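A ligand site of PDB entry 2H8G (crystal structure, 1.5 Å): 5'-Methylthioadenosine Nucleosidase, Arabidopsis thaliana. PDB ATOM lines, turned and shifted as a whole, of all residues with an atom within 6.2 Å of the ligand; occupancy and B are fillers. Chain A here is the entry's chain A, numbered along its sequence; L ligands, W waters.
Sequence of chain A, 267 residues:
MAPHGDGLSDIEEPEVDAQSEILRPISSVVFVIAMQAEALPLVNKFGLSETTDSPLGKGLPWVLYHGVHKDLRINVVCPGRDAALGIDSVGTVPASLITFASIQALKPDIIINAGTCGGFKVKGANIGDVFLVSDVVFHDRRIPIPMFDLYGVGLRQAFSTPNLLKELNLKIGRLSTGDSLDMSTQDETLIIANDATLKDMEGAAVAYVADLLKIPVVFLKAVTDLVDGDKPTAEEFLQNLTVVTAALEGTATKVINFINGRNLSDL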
ATOM      1  N   THR A 116       6.737 -14.731  -5.066  1.00  0.00           N
ATOM      2  CA  THR A 116       7.769 -14.974  -4.080  1.00  0.00           C
ATOM      3  C   THR A 116       8.844 -15.877  -4.670  1.00  0.00           C
ATOM      4  O   THR A 116       8.624 -16.563  -5.677  1.00  0.00           O
ATOM      5  CB  THR A 116       7.181 -15.631  -2.815  1.00  0.00           C
ATOM      6  OG1 THR A 116       6.379 -16.766  -3.178  1.00  0.00           O
ATOM      7  CG2 THR A 116       6.328 -14.646  -2.062  1.00  0.00           C
ATOM      8  N   CYS A 117      10.013 -15.897  -4.042  1.00  0.00           N
ATOM      9  CA  CYS A 117      11.111 -16.702  -4.543  1.00  0.00           C
ATOM     10  C   CYS A 117      12.151 -16.929  -3.460  1.00  0.00           C
ATOM     11  O   CYS A 117      12.085 -16.312  -2.388  1.00  0.00           O
ATOM     12  CB  CYS A 117      11.793 -15.993  -5.721  1.00  0.00           C
ATOM     13  SG  CYS A 117      12.688 -14.478  -5.249  1.00  0.00           S
ATOM     14  N   GLY A 118      13.099 -17.806  -3.755  1.00  0.00           N
ATOM     15  CA  GLY A 118      14.192 -18.040  -2.838  1.00  0.00           C
ATOM     16  C   GLY A 118      15.318 -17.133  -3.293  1.00  0.00           C
ATOM     17  O   GLY A 118      15.366 -16.729  -4.456  1.00  0.00           O
ATOM     18  N   GLY A 119      16.210 -16.785  -2.380  1.00  0.00           N
ATOM     19  CA  GLY A 119      17.319 -15.917  -2.736  1.00  0.00           C
ATOM     20  C   GLY A 119      18.620 -16.433  -2.176  1.00  0.00           C
ATOM     21  O   GLY A 119      18.645 -17.228  -1.231  1.00  0.00           O
ATOM     22  N   GLY A 178      12.835 -23.809 -11.771  1.00  0.00           N
ATOM     23  CA  GLY A 178      12.784 -25.255 -11.759  1.00  0.00           C
ATOM     24  C   GLY A 178      11.458 -25.657 -11.125  1.00  0.00           C
ATOM     25  O   GLY A 178      10.880 -24.875 -10.365  1.00  0.00           O
ATOM     26  N   SER A 180      10.910 -27.795  -8.771  1.00  0.00           N
ATOM     27  CA  SER A 180      11.033 -28.306  -7.414  1.00  0.00           C
ATOM     28  C   SER A 180      11.267 -27.138  -6.460  1.00  0.00           C
ATOM     29  O   SER A 180      11.966 -26.185  -6.790  1.00  0.00           O
ATOM     30  CB  SER A 180      12.174 -29.313  -7.311  1.00  0.00           C
ATOM     31  OG  SER A 180      11.895 -30.471  -8.070  1.00  0.00           O
ATOM     32  N   LEU A 181      10.652 -27.220  -5.279  1.00  0.00           N
ATOM     33  CA  LEU A 181      10.792 -26.174  -4.279  1.00  0.00           C
ATOM     34  C   LEU A 181      12.093 -26.396  -3.519  1.00  0.00           C
ATOM     35  O   LEU A 181      12.709 -25.435  -3.044  1.00  0.00           O
ATOM     36  CB  LEU A 181       9.603 -26.219  -3.321  1.00  0.00           C
ATOM     37  CG  LEU A 181       9.674 -25.260  -2.134  1.00  0.00           C
ATOM     38  CD1 LEU A 181       9.724 -23.825  -2.625  1.00  0.00           C
ATOM     39  CD2 LEU A 181       8.463 -25.471  -1.234  1.00  0.00           C
ATOM     40  N   ASP A 182      12.500 -27.641  -3.398  1.00  0.00           N
ATOM     41  CA  ASP A 182      13.745 -27.971  -2.722  1.00  0.00           C
ATOM     42  C   ASP A 182      14.862 -27.766  -3.736  1.00  0.00           C
ATOM     43  O   ASP A 182      14.623 -27.259  -4.836  1.00  0.00           O
ATOM     44  CB  ASP A 182      13.720 -29.426  -2.225  1.00  0.00           C
ATOM     45  CG  ASP A 182      13.708 -30.446  -3.348  1.00  0.00           C
ATOM     46  OD1 ASP A 182      13.415 -30.063  -4.506  1.00  0.00           O
ATOM     47  OD2 ASP A 182      13.977 -31.640  -3.092  1.00  0.00           O
ATOM     48  N   LYS A 199      15.690 -17.897  -7.111  1.00  0.00           N
ATOM     49  CA  LYS A 199      15.222 -19.221  -7.491  1.00  0.00           C
ATOM     50  C   LYS A 199      13.710 -19.291  -7.348  1.00  0.00           C
ATOM     51  O   LYS A 199      13.164 -18.942  -6.300  1.00  0.00           O
ATOM     52  CB  LYS A 199      15.895 -20.266  -6.602  1.00  0.00           C
ATOM     53  CG  LYS A 199      15.468 -21.709  -6.831  1.00  0.00           C
ATOM     54  CD  LYS A 199      16.155 -22.635  -5.825  1.00  0.00           C
ATOM     55  CE  LYS A 199      15.782 -24.087  -6.044  1.00  0.00           C
ATOM     56  NZ  LYS A 199      14.322 -24.333  -5.844  1.00  0.00           N
ATOM     57  N   ASP A 200      13.027 -19.724  -8.408  1.00  0.00           N
ATOM     58  CA  ASP A 200      11.565 -19.832  -8.350  1.00  0.00           C
ATOM     59  C   ASP A 200      11.065 -21.050  -9.121  1.00  0.00           C
ATOM     60  O   ASP A 200      11.857 -21.915  -9.499  1.00  0.00           O
ATOM     61  CB  ASP A 200      10.887 -18.566  -8.883  1.00  0.00           C
ATOM     62  CG  ASP A 200      10.871 -18.509 -10.398  1.00  0.00           C
ATOM     63  OD1 ASP A 200       9.998 -17.822 -10.958  1.00  0.00           O
ATOM     64  OD2 ASP A 200      11.744 -19.145 -11.026  1.00  0.00           O
ATOM     65  N   MET A 201       9.762 -21.111  -9.356  1.00  0.00           N
ATOM     66  CA  MET A 201       9.180 -22.247 -10.043  1.00  0.00           C
ATOM     67  C   MET A 201       8.377 -21.940 -11.304  1.00  0.00           C
ATOM     68  O   MET A 201       7.794 -22.856 -11.880  1.00  0.00           O
ATOM     69  CB  MET A 201       8.305 -23.045  -9.057  1.00  0.00           C
ATOM     70  CG  MET A 201       9.099 -23.655  -7.907  1.00  0.00           C
ATOM     71  SD  MET A 201       8.076 -24.299  -6.566  1.00  0.00           S
ATOM     72  CE  MET A 201       7.289 -25.647  -7.372  1.00  0.00           C
ATOM     73  N   ALA A 222       9.885 -11.434  -4.936  1.00  0.00           N
ATOM     74  CA  ALA A 222      10.095 -11.118  -3.532  1.00  0.00           C
ATOM     75  C   ALA A 222      10.678 -12.308  -2.758  1.00  0.00           C
ATOM     76  O   ALA A 222      10.089 -13.388  -2.726  1.00  0.00           O
ATOM     77  CB  ALA A 222       8.780 -10.669  -2.912  1.00  0.00           C
ATOM     78  N   THR A 224      11.462 -14.753   0.031  1.00  0.00           N
ATOM     79  CA  THR A 224      10.845 -15.286   1.246  1.00  0.00           C
ATOM     80  C   THR A 224      11.782 -16.186   2.037  1.00  0.00           C
ATOM     81  O   THR A 224      11.552 -16.455   3.220  1.00  0.00           O
ATOM     82  CB  THR A 224       9.577 -16.117   0.928  1.00  0.00           C
ATOM     83  OG1 THR A 224       9.863 -17.059  -0.114  1.00  0.00           O
ATOM     84  CG2 THR A 224       8.435 -15.205   0.504  1.00  0.00           C
ATOM     85  N   ASP A 225      12.838 -16.659   1.390  1.00  0.00           N
ATOM     86  CA  ASP A 225      13.763 -17.550   2.068  1.00  0.00           C
ATOM     87  C   ASP A 225      15.155 -17.480   1.442  1.00  0.00           C
ATOM     88  O   ASP A 225      15.295 -17.139   0.270  1.00  0.00           O
ATOM     89  CB  ASP A 225      13.251 -18.997   2.011  1.00  0.00           C
ATOM     90  CG  ASP A 225      12.928 -19.444   0.595  1.00  0.00           C
ATOM     91  OD1 ASP A 225      11.915 -18.986   0.039  1.00  0.00           O
ATOM     92  OD2 ASP A 225      13.704 -20.246   0.027  1.00  0.00           O
ATOM     93  N   VAL A 227      18.191 -19.597   0.285  1.00  0.00           N
ATOM     94  CA  VAL A 227      18.590 -20.946  -0.083  1.00  0.00           C
ATOM     95  C   VAL A 227      19.917 -21.361   0.544  1.00  0.00           C
ATOM     96  O   VAL A 227      20.129 -22.531   0.845  1.00  0.00           O
ATOM     97  CB  VAL A 227      18.658 -21.097  -1.613  1.00  0.00           C
ATOM     98  CG1 VAL A 227      19.006 -22.534  -1.981  1.00  0.00           C
ATOM     99  CG2 VAL A 227      17.316 -20.721  -2.222  1.00  0.00           C
ATOM    100  N   THR A 233      14.040 -24.693   3.802  1.00  0.00           N
ATOM    101  CA  THR A 233      13.411 -23.908   2.749  1.00  0.00           C
ATOM    102  C   THR A 233      11.899 -23.783   2.865  1.00  0.00           C
ATOM    103  O   THR A 233      11.377 -22.659   2.918  1.00  0.00           O
ATOM    104  CB  THR A 233      13.750 -24.482   1.359  1.00  0.00           C
ATOM    105  OG1 THR A 233      15.144 -24.302   1.100  1.00  0.00           O
ATOM    106  CG2 THR A 233      12.938 -23.789   0.272  1.00  0.00           C
ATOM    107  N   PHE A 237      10.087 -20.328   3.841  1.00  0.00           N
ATOM    108  CA  PHE A 237       9.240 -19.827   2.760  1.00  0.00           C
ATOM    109  C   PHE A 237       7.837 -19.514   3.267  1.00  0.00           C
ATOM    110  O   PHE A 237       7.340 -18.404   3.114  1.00  0.00           O
ATOM    111  CB  PHE A 237       9.189 -20.877   1.638  1.00  0.00           C
ATOM    112  CG  PHE A 237       8.018 -20.730   0.705  1.00  0.00           C
ATOM    113  CD1 PHE A 237       7.693 -19.508   0.143  1.00  0.00           C
ATOM    114  CD2 PHE A 237       7.257 -21.851   0.366  1.00  0.00           C
ATOM    115  CE1 PHE A 237       6.627 -19.392  -0.759  1.00  0.00           C
ATOM    116  CE2 PHE A 237       6.188 -21.757  -0.525  1.00  0.00           C
ATOM    117  CZ  PHE A 237       5.883 -20.520  -1.088  1.00  0.00           C
HETATM  118  N1  LIG L   1       9.547 -19.920  -3.858  1.00  0.00           N
HETATM  119  C1  LIG L   1       9.912 -19.427  -2.655  1.00  0.00           C
HETATM  120  N2  LIG L   1      11.104 -19.900  -2.211  1.00  0.00           N
HETATM  121  C2  LIG L   1      11.509 -20.740  -3.213  1.00  0.00           C
HETATM  122  C3  LIG L   1      12.672 -21.577  -3.403  1.00  0.00           C
HETATM  123  N3  LIG L   1      13.637 -21.627  -2.497  1.00  0.00           N
HETATM  124  N4  LIG L   1      12.755 -22.333  -4.595  1.00  0.00           N
HETATM  125  C4  LIG L   1      11.743 -22.263  -5.532  1.00  0.00           C
HETATM  126  N5  LIG L   1      10.590 -21.493  -5.423  1.00  0.00           N
HETATM  127  C5  LIG L   1      10.551 -20.762  -4.238  1.00  0.00           C
HETATM  128  O   HOH W   1       7.107 -18.910  -5.089  1.00  0.00           O
HETATM  129  O   HOH W   2      15.160 -24.227  -2.800  1.00  0.00           O
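The backbone carbonyl oxygen of Leu 181 sits close to a nitrogen (N4) of the ligand, 3.5 Å away.
Thr 116 touches the ligand.
Cys 117 touches the ligand (C to N2, 3.4 Å).
Asp 200 touches the ligand.
Met 201 touches the ligand.
Thr 224 touches the ligand.
Val 227 touches the ligand.
Thr 233 touches the ligand (CG2 to N3, 3.6 Å).
Phe 237 touches the ligand (CD1 to C1, 3.6 Å).
The backbone carbonyl oxygen of Asp 225 lies within hydrogen-bond range of the backbone NH of Gly 119, at 2.8 Å.
N of Cys 117 sits at hydrogen-bond distance from O of Ala 222 (2.8 Å).
The side-chain amino group of Lys 199 is in hydrogen-bond range of the backbone carbonyl oxygen of Ser 180 (3.1 Å).
The backbone carbonyl oxygen of Cys 117 sits at hydrogen-bond distance from the backbone NH of Thr 224 (2.9 Å).
O of Lys 199 is in hydrogen-bond range of N of Gly 118 (2.8 Å).
The backbone NH (N) of Gly 178 sits at hydrogen-bond distance from the backbone carbonyl oxygen (O) of Asp 200, at 3.1 Å.
The side-chain amino group (NZ) of Lys 199 lies within hydrogen-bond range of the backbone carbonyl oxygen (O) of Asp 182, 3.1 Å away.
The side-chain carboxylate (OD1) of Asp 225 sits at hydrogen-bond distance from the side-chain hydroxyl (OG1) of Thr 224 (2.8 Å).
Water W1 lies within hydrogen-bond range of O of Thr 116 (2.9 Å) and N1 of the ligand (2.9 Å).
Water W2 lies within hydrogen-bond range of the backbone carbonyl oxygen of Leu 181, a nitrogen (N3) of the ligand and the side-chain amino group of Lys 199.
NZ of Lys 199 is in hydrogen-bond range of N4 of the ligand (2.8 Å).
N2 of the ligand is in hydrogen-bond range of N of Gly 118, at 3.3 Å.
The side-chain carboxylate of Asp 225 sits at hydrogen-bond distance from a nitrogen (N2) of the ligand.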
